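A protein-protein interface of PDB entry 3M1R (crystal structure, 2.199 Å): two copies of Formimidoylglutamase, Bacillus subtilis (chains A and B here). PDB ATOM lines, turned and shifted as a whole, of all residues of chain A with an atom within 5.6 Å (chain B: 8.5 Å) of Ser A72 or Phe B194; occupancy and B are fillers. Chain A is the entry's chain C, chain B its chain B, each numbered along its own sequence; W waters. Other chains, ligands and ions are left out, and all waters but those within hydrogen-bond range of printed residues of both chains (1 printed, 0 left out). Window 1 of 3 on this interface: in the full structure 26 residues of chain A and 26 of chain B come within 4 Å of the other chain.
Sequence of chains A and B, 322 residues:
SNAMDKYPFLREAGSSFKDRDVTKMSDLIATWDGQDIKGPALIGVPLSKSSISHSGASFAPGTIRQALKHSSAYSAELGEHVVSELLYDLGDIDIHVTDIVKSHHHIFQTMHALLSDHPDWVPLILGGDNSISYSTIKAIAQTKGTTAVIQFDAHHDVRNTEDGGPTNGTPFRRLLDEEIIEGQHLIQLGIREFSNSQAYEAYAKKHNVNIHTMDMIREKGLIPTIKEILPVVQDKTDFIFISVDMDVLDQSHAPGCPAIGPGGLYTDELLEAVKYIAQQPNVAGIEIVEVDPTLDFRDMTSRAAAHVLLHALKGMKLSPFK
The backbone carbonyl oxygen (O) of Asn B196 lies within hydrogen-bond range of the side-chain hydroxyl (OG) of Ser A72 (2.6 Å).
The side-chain carboxylate (OE1) of Glu B193 lies within hydrogen-bond range of the backbone NH (N) of Ala A76, 3.1 Å away.
NZ of Lys A314 lies within salt-bridge range of OE2 of Glu B193 (2.6 Å).
The side-chain hydroxyl of Ser A75 sits at hydrogen-bond distance from the side-chain carboxylate of Glu B193, at 2.7 Å.
The side-chain hydroxyl of Tyr A74 sits at hydrogen-bond distance from the side-chain carboxylate of Glu B201 (2.7 Å).
CB of Ser A72 touches O of Phe B194 (3.6 Å).
Tyr A74 touches Phe B194.
Tyr A74 touches Asn B196 (CB to O, 3.6 Å).
Tyr A74 touches Ser B197 (CD2 to C, 3.8 Å).
N of Gln B198 touches CD2 of Tyr A74 (3.5 Å).
CB of Ser A75 touches CE2 of Phe B194, at 3.9 Å.
Ala A76 touches Glu B201.
His A307 touches Pro B262 (CD2 to CD, 3.7 Å).
CZ of Phe B194 touches O of Leu A310, at 3.9 Å.
Phe B194 touches His A311.
Ser A72 touches just these residues of chain B: Phe B194 (3.6 Å) and Asn B196 (2.6 Å).
Of chain A, only Ser A72 (3.6 Å), Tyr A74 (3.5 Å), Ser A75 (3.9 Å), Val A82 (3.6 Å), Leu A310 (3.9 Å) and His A311 (3.8 Å) come within 4 Å of Phe B194.
Of the printed residues of chain B, Tyr A74 touches Phe B194 (3.5 Å), Asn B196 (3.6 Å), Ser B197 (3.8 Å), Gln B198 (3.5 Å) and Glu B201 (2.7 Å).
Of the printed residues of chain B, Leu A310 touches Phe B194 (3.9 Å).
Of the printed residues of chain B, Ala A76 touches Glu B193 and Glu B201.
Printed residues of chain A within 4 Å of Glu B201: Tyr A74 (2.7 Å) and Ala A76 (3.3 Å).
Of the printed residues of chain B, Val A82 touches Phe B194.
The nearest residue of chain B that does not touch Ser A72 is Ser B197 (4.3 Å).
No position is printed for both chains.
Of the 16 printed residues of chain A, 9 touch a printed residue of chain B.
Hydrophobic or aromatic side chains of chain A within 4 Å of the printed part of chain B: Tyr A74, Ala A76, Val A82, His A307, Leu A310 and His A311.
Hydrophobic or aromatic side chains of chain B within 4 Å of the printed part of chain A: Phe B194 and Pro B262.
Among the printed residues, 16 pairs touch across the chains.
Among the printed residues, Asp or Glu carboxylates within 4 Å of a Lys or Arg side-chain nitrogen of the other chain: Lys A314 with Glu B193 (2.6 Å).
O of Ala B154 lies within hydrogen-bond range of ND2 of Asn B196 (2.9 Å).
The backbone carbonyl oxygen (O) of Arg B192 lies within hydrogen-bond range of the side-chain amide nitrogen (ND2) of Asn B196, 3.3 Å away.
The backbone carbonyl oxygen of Ala A73 sits at hydrogen-bond distance from the backbone NH of Val A82.
The backbone NH (N) of Tyr A74 is in hydrogen-bond range of the side-chain hydroxyl (OG) of Ser A72 (3.1 Å).
Water W1 bridges the backbone NH of Phe B194 and the backbone carbonyl oxygen of Tyr A74.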
ATOM      1  N   THR A  23       9.413  32.301  -4.593  1.00  0.00           N
ATOM      2  CA  THR A  23       8.382  32.998  -5.332  1.00  0.00           C
ATOM      3  C   THR A  23       6.985  32.643  -4.802  1.00  0.00           C
ATOM      4  O   THR A  23       6.480  31.533  -4.987  1.00  0.00           O
ATOM      5  CB  THR A  23       8.547  32.789  -6.848  1.00  0.00           C
ATOM      6  OG1 THR A  23       7.336  33.143  -7.525  1.00  0.00           O
ATOM      7  CG2 THR A  23       8.918  31.350  -7.145  1.00  0.00           C
ATOM      8  N   LYS A  24       6.392  33.603  -4.102  1.00  0.00           N
ATOM      9  CA  LYS A  24       5.065  33.449  -3.533  1.00  0.00           C
ATOM     10  C   LYS A  24       4.017  33.926  -4.527  1.00  0.00           C
ATOM     11  O   LYS A  24       4.341  34.580  -5.522  1.00  0.00           O
ATOM     12  CB  LYS A  24       4.960  34.258  -2.240  1.00  0.00           C
ATOM     13  CG  LYS A  24       5.615  33.598  -1.045  1.00  0.00           C
ATOM     14  CD  LYS A  24       6.070  34.622   0.003  1.00  0.00           C
ATOM     15  CE  LYS A  24       4.933  35.485   0.532  1.00  0.00           C
ATOM     16  NZ  LYS A  24       5.393  36.367   1.664  1.00  0.00           N
ATOM     17  N   MET A  25       2.761  33.598  -4.260  1.00  0.00           N
ATOM     18  CA  MET A  25       1.675  34.043  -5.122  1.00  0.00           C
ATOM     19  C   MET A  25       1.588  35.567  -5.127  1.00  0.00           C
ATOM     20  O   MET A  25       1.147  36.170  -6.116  1.00  0.00           O
ATOM     21  CB  MET A  25       0.343  33.430  -4.675  1.00  0.00           C
ATOM     22  CG  MET A  25       0.233  31.944  -5.006  1.00  0.00           C
ATOM     23  SD  MET A  25       0.218  31.651  -6.953  1.00  0.00           S
ATOM     24  CE  MET A  25      -1.451  32.539  -7.353  1.00  0.00           C
ATOM     25  N   LEU A  68      -3.729  33.054   0.208  1.00  0.00           N
ATOM     26  CA  LEU A  68      -3.217  32.707  -1.123  1.00  0.00           C
ATOM     27  C   LEU A  68      -1.866  33.396  -1.374  1.00  0.00           C
ATOM     28  O   LEU A  68      -0.894  32.765  -1.817  1.00  0.00           O
ATOM     29  CB  LEU A  68      -4.206  33.126  -2.215  1.00  0.00           C
ATOM     30  CG  LEU A  68      -3.870  32.705  -3.651  1.00  0.00           C
ATOM     31  CD1 LEU A  68      -3.633  31.175  -3.736  1.00  0.00           C
ATOM     32  CD2 LEU A  68      -4.970  33.150  -4.621  1.00  0.00           C
ATOM     33  N   HIS A  70       0.390  34.532   0.600  1.00  0.00           N
ATOM     34  CA  HIS A  70       1.502  34.053   1.413  1.00  0.00           C
ATOM     35  C   HIS A  70       1.934  32.623   1.091  1.00  0.00           C
ATOM     36  O   HIS A  70       2.897  32.126   1.667  1.00  0.00           O
ATOM     37  CB  HIS A  70       1.207  34.226   2.908  1.00  0.00           C
ATOM     38  CG  HIS A  70       1.367  35.638   3.382  1.00  0.00           C
ATOM     39  ND1 HIS A  70       0.300  36.497   3.548  1.00  0.00           N
ATOM     40  CD2 HIS A  70       2.475  36.357   3.687  1.00  0.00           C
ATOM     41  CE1 HIS A  70       0.742  37.673   3.955  1.00  0.00           C
ATOM     42  NE2 HIS A  70       2.059  37.614   4.048  1.00  0.00           N
ATOM     43  N   SER A  71       1.245  31.983   0.150  1.00  0.00           N
ATOM     44  CA  SER A  71       1.608  30.636  -0.271  1.00  0.00           C
ATOM     45  C   SER A  71       2.661  30.670  -1.389  1.00  0.00           C
ATOM     46  O   SER A  71       2.734  31.633  -2.149  1.00  0.00           O
ATOM     47  CB  SER A  71       0.372  29.873  -0.773  1.00  0.00           C
ATOM     48  OG  SER A  71      -0.651  29.844   0.209  1.00  0.00           O
ATOM     49  N   SER A  72       3.461  29.607  -1.472  1.00  0.00           N
ATOM     50  CA  SER A  72       4.308  29.346  -2.630  1.00  0.00           C
ATOM     51  C   SER A  72       3.490  29.043  -3.883  1.00  0.00           C
ATOM     52  O   SER A  72       2.458  28.376  -3.819  1.00  0.00           O
ATOM     53  CB  SER A  72       5.235  28.166  -2.353  1.00  0.00           C
ATOM     54  OG  SER A  72       5.998  27.843  -3.508  1.00  0.00           O
ATOM     55  N   ALA A  73       3.975  29.524  -5.024  1.00  0.00           N
ATOM     56  CA  ALA A  73       3.338  29.288  -6.310  1.00  0.00           C
ATOM     57  C   ALA A  73       3.874  28.012  -6.957  1.00  0.00           C
ATOM     58  O   ALA A  73       3.386  27.577  -7.997  1.00  0.00           O
ATOM     59  CB  ALA A  73       3.582  30.485  -7.231  1.00  0.00           C
ATOM     60  N   TYR A  74       4.880  27.413  -6.338  1.00  0.00           N
ATOM     61  CA  TYR A  74       5.589  26.305  -6.962  1.00  0.00           C
ATOM     62  C   TYR A  74       4.991  24.938  -6.632  1.00  0.00           C
ATOM     63  O   TYR A  74       4.859  24.569  -5.461  1.00  0.00           O
ATOM     64  CB  TYR A  74       7.072  26.322  -6.582  1.00  0.00           C
ATOM     65  CG  TYR A  74       7.832  25.150  -7.164  1.00  0.00           C
ATOM     66  CD1 TYR A  74       8.072  25.071  -8.526  1.00  0.00           C
ATOM     67  CD2 TYR A  74       8.295  24.116  -6.359  1.00  0.00           C
ATOM     68  CE1 TYR A  74       8.749  24.002  -9.080  1.00  0.00           C
ATOM     69  CE2 TYR A  74       8.989  23.039  -6.905  1.00  0.00           C
ATOM     70  CZ  TYR A  74       9.209  22.990  -8.271  1.00  0.00           C
ATOM     71  OH  TYR A  74       9.885  21.935  -8.846  1.00  0.00           O
ATOM     72  N   SER A  75       4.650  24.188  -7.681  1.00  0.00           N
ATOM     73  CA  SER A  75       4.165  22.821  -7.546  1.00  0.00           C
ATOM     74  C   SER A  75       5.292  21.818  -7.771  1.00  0.00           C
ATOM     75  O   SER A  75       5.801  21.691  -8.882  1.00  0.00           O
ATOM     76  CB  SER A  75       3.039  22.563  -8.549  1.00  0.00           C
ATOM     77  OG  SER A  75       2.752  21.179  -8.660  1.00  0.00           O
ATOM     78  N   ALA A  76       5.684  21.107  -6.722  1.00  0.00           N
ATOM     79  CA  ALA A  76       6.723  20.091  -6.860  1.00  0.00           C
ATOM     80  C   ALA A  76       6.292  19.040  -7.870  1.00  0.00           C
ATOM     81  O   ALA A  76       7.123  18.480  -8.589  1.00  0.00           O
ATOM     82  CB  ALA A  76       7.037  19.443  -5.509  1.00  0.00           C
ATOM     83  N   VAL A  82       2.333  27.290 -10.760  1.00  0.00           N
ATOM     84  CA  VAL A  82       0.966  27.104 -11.239  1.00  0.00           C
ATOM     85  C   VAL A  82       0.523  28.304 -12.045  1.00  0.00           C
ATOM     86  O   VAL A  82      -0.520  28.287 -12.690  1.00  0.00           O
ATOM     87  CB  VAL A  82      -0.015  26.898 -10.095  1.00  0.00           C
ATOM     88  CG1 VAL A  82       0.019  25.459  -9.633  1.00  0.00           C
ATOM     89  CG2 VAL A  82       0.291  27.872  -8.972  1.00  0.00           C
ATOM     90  N   HIS A 307      -5.776  26.852  -0.930  1.00  0.00           N
ATOM     91  CA  HIS A 307      -5.282  25.640  -1.586  1.00  0.00           C
ATOM     92  C   HIS A 307      -6.250  25.073  -2.623  1.00  0.00           C
ATOM     93  O   HIS A 307      -5.826  24.527  -3.642  1.00  0.00           O
ATOM     94  CB  HIS A 307      -4.895  24.585  -0.559  1.00  0.00           C
ATOM     95  CG  HIS A 307      -3.599  24.880   0.107  1.00  0.00           C
ATOM     96  ND1 HIS A 307      -2.459  24.147  -0.135  1.00  0.00           N
ATOM     97  CD2 HIS A 307      -3.242  25.873   0.953  1.00  0.00           C
ATOM     98  CE1 HIS A 307      -1.461  24.659   0.563  1.00  0.00           C
ATOM     99  NE2 HIS A 307      -1.909  25.705   1.230  1.00  0.00           N
ATOM    100  N   LEU A 310      -5.271  26.974  -5.527  1.00  0.00           N
ATOM    101  CA  LEU A 310      -3.955  26.557  -5.992  1.00  0.00           C
ATOM    102  C   LEU A 310      -4.073  25.260  -6.796  1.00  0.00           C
ATOM    103  O   LEU A 310      -3.464  25.122  -7.857  1.00  0.00           O
ATOM    104  CB  LEU A 310      -2.989  26.390  -4.817  1.00  0.00           C
ATOM    105  CG  LEU A 310      -2.420  27.658  -4.154  1.00  0.00           C
ATOM    106  CD1 LEU A 310      -1.844  27.337  -2.754  1.00  0.00           C
ATOM    107  CD2 LEU A 310      -1.355  28.373  -5.035  1.00  0.00           C
ATOM    108  N   HIS A 311      -4.861  24.310  -6.291  1.00  0.00           N
ATOM    109  CA  HIS A 311      -5.057  23.030  -6.978  1.00  0.00           C
ATOM    110  C   HIS A 311      -5.909  23.146  -8.251  1.00  0.00           C
ATOM    111  O   HIS A 311      -5.651  22.450  -9.215  1.00  0.00           O
ATOM    112  CB  HIS A 311      -5.557  21.919  -6.030  1.00  0.00           C
ATOM    113  CG  HIS A 311      -4.499  21.407  -5.100  1.00  0.00           C
ATOM    114  ND1 HIS A 311      -3.775  20.260  -5.351  1.00  0.00           N
ATOM    115  CD2 HIS A 311      -4.016  21.904  -3.935  1.00  0.00           C
ATOM    116  CE1 HIS A 311      -2.900  20.065  -4.379  1.00  0.00           C
ATOM    117  NE2 HIS A 311      -3.026  21.048  -3.504  1.00  0.00           N
ATOM    118  N   LYS A 314      -3.470  24.478 -10.692  1.00  0.00           N
ATOM    119  CA  LYS A 314      -2.592  23.376 -11.057  1.00  0.00           C
ATOM    120  C   LYS A 314      -3.219  22.498 -12.140  1.00  0.00           C
ATOM    121  O   LYS A 314      -2.570  22.188 -13.135  1.00  0.00           O
ATOM    122  CB  LYS A 314      -2.216  22.560  -9.820  1.00  0.00           C
ATOM    123  CG  LYS A 314      -1.397  21.301 -10.080  1.00  0.00           C
ATOM    124  CD  LYS A 314      -1.148  20.626  -8.745  1.00  0.00           C
ATOM    125  CE  LYS A 314      -0.743  19.179  -8.882  1.00  0.00           C
ATOM    126  NZ  LYS A 314      -0.653  18.521  -7.540  1.00  0.00           N
ATOM    127  N   ALA B 154       7.209  19.376   6.317  1.00  0.00           N
ATOM    128  CA  ALA B 154       6.599  19.833   5.070  1.00  0.00           C
ATOM    129  C   ALA B 154       7.615  20.606   4.218  1.00  0.00           C
ATOM    130  O   ALA B 154       7.486  20.678   2.996  1.00  0.00           O
ATOM    131  CB  ALA B 154       5.382  20.696   5.343  1.00  0.00           C
ATOM    132  N   HIS B 155       8.624  21.183   4.861  1.00  0.00           N
ATOM    133  CA  HIS B 155       9.564  22.058   4.153  1.00  0.00           C
ATOM    134  C   HIS B 155      10.973  21.484   4.087  1.00  0.00           C
ATOM    135  O   HIS B 155      11.393  20.733   4.971  1.00  0.00           O
ATOM    136  CB  HIS B 155       9.597  23.447   4.803  1.00  0.00           C
ATOM    137  CG  HIS B 155       8.243  23.985   5.114  1.00  0.00           C
ATOM    138  ND1 HIS B 155       7.600  23.729   6.304  1.00  0.00           N
ATOM    139  CD2 HIS B 155       7.384  24.731   4.375  1.00  0.00           C
ATOM    140  CE1 HIS B 155       6.412  24.307   6.297  1.00  0.00           C
ATOM    141  NE2 HIS B 155       6.255  24.915   5.136  1.00  0.00           N
ATOM    142  N   ARG B 159      16.836  27.138   3.193  1.00  0.00           N
ATOM    143  CA  ARG B 159      16.795  28.555   2.859  1.00  0.00           C
ATOM    144  C   ARG B 159      18.180  29.193   2.949  1.00  0.00           C
ATOM    145  O   ARG B 159      18.951  28.894   3.861  1.00  0.00           O
ATOM    146  CB  ARG B 159      15.863  29.304   3.813  1.00  0.00           C
ATOM    147  CG  ARG B 159      14.372  29.085   3.611  1.00  0.00           C
ATOM    148  CD  ARG B 159      13.628  30.176   4.373  1.00  0.00           C
ATOM    149  NE  ARG B 159      12.177  30.093   4.270  1.00  0.00           N
ATOM    150  CZ  ARG B 159      11.416  31.019   3.696  1.00  0.00           C
ATOM    151  NH1 ARG B 159      11.978  32.094   3.154  1.00  0.00           N
ATOM    152  NH2 ARG B 159      10.093  30.874   3.668  1.00  0.00           N
ATOM    153  N   ILE B 191       7.534  16.140   2.657  1.00  0.00           N
ATOM    154  CA  ILE B 191       7.681  17.358   1.873  1.00  0.00           C
ATOM    155  C   ILE B 191       6.403  17.628   1.100  1.00  0.00           C
ATOM    156  O   ILE B 191       5.897  16.763   0.389  1.00  0.00           O
ATOM    157  CB  ILE B 191       8.883  17.287   0.900  1.00  0.00           C
ATOM    158  CG1 ILE B 191      10.205  17.243   1.672  1.00  0.00           C
ATOM    159  CG2 ILE B 191       8.864  18.481  -0.038  1.00  0.00           C
ATOM    160  CD1 ILE B 191      10.398  18.380   2.667  1.00  0.00           C
ATOM    161  N   ARG B 192       5.881  18.839   1.215  1.00  0.00           N
ATOM    162  CA  ARG B 192       4.474  19.043   0.880  1.00  0.00           C
ATOM    163  C   ARG B 192       4.283  19.981  -0.300  1.00  0.00           C
ATOM    164  O   ARG B 192       4.975  20.986  -0.426  1.00  0.00           O
ATOM    165  CB  ARG B 192       3.764  19.601   2.101  1.00  0.00           C
ATOM    166  CG  ARG B 192       2.303  19.304   2.225  1.00  0.00           C
ATOM    167  CD  ARG B 192       2.020  19.157   3.712  1.00  0.00           C
ATOM    168  NE  ARG B 192       1.250  20.263   4.203  1.00  0.00           N
ATOM    169  CZ  ARG B 192       1.072  20.557   5.488  1.00  0.00           C
ATOM    170  NH1 ARG B 192       0.322  21.601   5.798  1.00  0.00           N
ATOM    171  NH2 ARG B 192       1.626  19.826   6.452  1.00  0.00           N
ATOM    172  N   GLU B 193       3.324  19.643  -1.149  1.00  0.00           N
ATOM    173  CA  GLU B 193       2.993  20.418  -2.336  1.00  0.00           C
ATOM    174  C   GLU B 193       2.515  21.823  -1.963  1.00  0.00           C
ATOM    175  O   GLU B 193       1.608  21.977  -1.141  1.00  0.00           O
ATOM    176  CB  GLU B 193       1.914  19.675  -3.141  1.00  0.00           C
ATOM    177  CG  GLU B 193       1.391  20.412  -4.354  1.00  0.00           C
ATOM    178  CD  GLU B 193       2.052  19.977  -5.652  1.00  0.00           C
ATOM    179  OE1 GLU B 193       3.245  19.614  -5.627  1.00  0.00           O
ATOM    180  OE2 GLU B 193       1.370  19.997  -6.701  1.00  0.00           O
ATOM    181  N   PHE B 194       3.124  22.825  -2.601  1.00  0.00           N
ATOM    182  CA  PHE B 194       2.908  24.254  -2.328  1.00  0.00           C
ATOM    183  C   PHE B 194       3.498  24.743  -1.002  1.00  0.00           C
ATOM    184  O   PHE B 194       3.213  25.850  -0.559  1.00  0.00           O
ATOM    185  CB  PHE B 194       1.431  24.656  -2.463  1.00  0.00           C
ATOM    186  CG  PHE B 194       0.889  24.428  -3.835  1.00  0.00           C
ATOM    187  CD1 PHE B 194      -0.104  23.488  -4.059  1.00  0.00           C
ATOM    188  CD2 PHE B 194       1.420  25.109  -4.919  1.00  0.00           C
ATOM    189  CE1 PHE B 194      -0.570  23.255  -5.342  1.00  0.00           C
ATOM    190  CE2 PHE B 194       0.948  24.882  -6.202  1.00  0.00           C
ATOM    191  CZ  PHE B 194      -0.041  23.958  -6.411  1.00  0.00           C
ATOM    192  N   SER B 195       4.332  23.928  -0.367  1.00  0.00           N
ATOM    193  CA  SER B 195       5.005  24.416   0.833  1.00  0.00           C
ATOM    194  C   SER B 195       6.448  24.825   0.534  1.00  0.00           C
ATOM    195  O   SER B 195       7.153  25.246   1.422  1.00  0.00           O
ATOM    196  CB  SER B 195       4.990  23.361   1.938  1.00  0.00           C
ATOM    197  OG  SER B 195       3.685  23.146   2.415  1.00  0.00           O
ATOM    198  N   ASN B 196       6.886  24.695  -0.714  1.00  0.00           N
ATOM    199  CA  ASN B 196       8.303  24.864  -1.017  1.00  0.00           C
ATOM    200  C   ASN B 196       8.582  25.666  -2.282  1.00  0.00           C
ATOM    201  O   ASN B 196       7.684  25.905  -3.090  1.00  0.00           O
ATOM    202  CB  ASN B 196       8.976  23.489  -1.101  1.00  0.00           C
ATOM    203  CG  ASN B 196       8.997  22.780   0.236  1.00  0.00           C
ATOM    204  OD1 ASN B 196       9.791  23.119   1.129  1.00  0.00           O
ATOM    205  ND2 ASN B 196       8.093  21.816   0.404  1.00  0.00           N
ATOM    206  N   SER B 197       9.834  26.072  -2.459  1.00  0.00           N
ATOM    207  CA  SER B 197      10.192  26.842  -3.640  1.00  0.00           C
ATOM    208  C   SER B 197      11.065  26.056  -4.625  1.00  0.00           C
ATOM    209  O   SER B 197      11.829  25.169  -4.237  1.00  0.00           O
ATOM    210  CB  SER B 197      10.900  28.118  -3.236  1.00  0.00           C
ATOM    211  OG  SER B 197      12.272  27.850  -3.021  1.00  0.00           O
ATOM    212  N   GLN B 198      10.948  26.399  -5.904  1.00  0.00           N
ATOM    213  CA  GLN B 198      11.752  25.762  -6.939  1.00  0.00           C
ATOM    214  C   GLN B 198      13.249  25.730  -6.638  1.00  0.00           C
ATOM    215  O   GLN B 198      13.895  24.700  -6.814  1.00  0.00           O
ATOM    216  CB  GLN B 198      11.525  26.432  -8.291  1.00  0.00           C
ATOM    217  CG  GLN B 198      11.947  25.552  -9.451  1.00  0.00           C
ATOM    218  CD  GLN B 198      11.748  26.212 -10.795  1.00  0.00           C
ATOM    219  OE1 GLN B 198      11.742  27.446 -10.903  1.00  0.00           O
ATOM    220  NE2 GLN B 198      11.591  25.395 -11.836  1.00  0.00           N
ATOM    221  N   ALA B 199      13.803  26.851  -6.188  1.00  0.00           N
ATOM    222  CA  ALA B 199      15.249  26.949  -5.988  1.00  0.00           C
ATOM    223  C   ALA B 199      15.741  26.075  -4.835  1.00  0.00           C
ATOM    224  O   ALA B 199      16.869  25.575  -4.871  1.00  0.00           O
ATOM    225  CB  ALA B 199      15.670  28.401  -5.770  1.00  0.00           C
ATOM    226  N   GLU B 201      14.179  23.217  -3.551  1.00  0.00           N
ATOM    227  CA  GLU B 201      14.064  21.843  -4.002  1.00  0.00           C
ATOM    228  C   GLU B 201      15.302  21.471  -4.827  1.00  0.00           C
ATOM    229  O   GLU B 201      15.822  20.361  -4.708  1.00  0.00           O
ATOM    230  CB  GLU B 201      12.798  21.682  -4.835  1.00  0.00           C
ATOM    231  CG  GLU B 201      12.645  20.311  -5.471  1.00  0.00           C
ATOM    232  CD  GLU B 201      11.395  20.200  -6.312  1.00  0.00           C
ATOM    233  OE1 GLU B 201      10.300  20.036  -5.735  1.00  0.00           O
ATOM    234  OE2 GLU B 201      11.506  20.276  -7.555  1.00  0.00           O
ATOM    235  N   ASP B 215       2.689  13.107  -1.463  1.00  0.00           N
ATOM    236  CA  ASP B 215       2.124  12.331  -2.560  1.00  0.00           C
ATOM    237  C   ASP B 215       2.729  10.938  -2.622  1.00  0.00           C
ATOM    238  O   ASP B 215       2.010   9.948  -2.709  1.00  0.00           O
ATOM    239  CB  ASP B 215       2.317  13.044  -3.893  1.00  0.00           C
ATOM    240  CG  ASP B 215       1.287  14.117  -4.129  1.00  0.00           C
ATOM    241  OD1 ASP B 215       0.229  14.077  -3.465  1.00  0.00           O
ATOM    242  OD2 ASP B 215       1.530  14.997  -4.983  1.00  0.00           O
ATOM    243  N   GLY B 261      -1.039  24.137   7.144  1.00  0.00           N
ATOM    244  CA  GLY B 261      -1.765  24.032   5.893  1.00  0.00           C
ATOM    245  C   GLY B 261      -2.453  22.688   5.831  1.00  0.00           C
ATOM    246  O   GLY B 261      -2.172  21.822   6.658  1.00  0.00           O
ATOM    247  N   PRO B 262      -3.336  22.493   4.834  1.00  0.00           N
ATOM    248  CA  PRO B 262      -4.014  21.204   4.662  1.00  0.00           C
ATOM    249  C   PRO B 262      -3.109  20.261   3.899  1.00  0.00           C
ATOM    250  O   PRO B 262      -2.165  20.724   3.241  1.00  0.00           O
ATOM    251  CB  PRO B 262      -5.241  21.572   3.833  1.00  0.00           C
ATOM    252  CG  PRO B 262      -4.737  22.701   2.949  1.00  0.00           C
ATOM    253  CD  PRO B 262      -3.705  23.464   3.785  1.00  0.00           C
HETATM  254  O   HOH W   1       5.737  22.540  -3.499  1.00  0.00           O
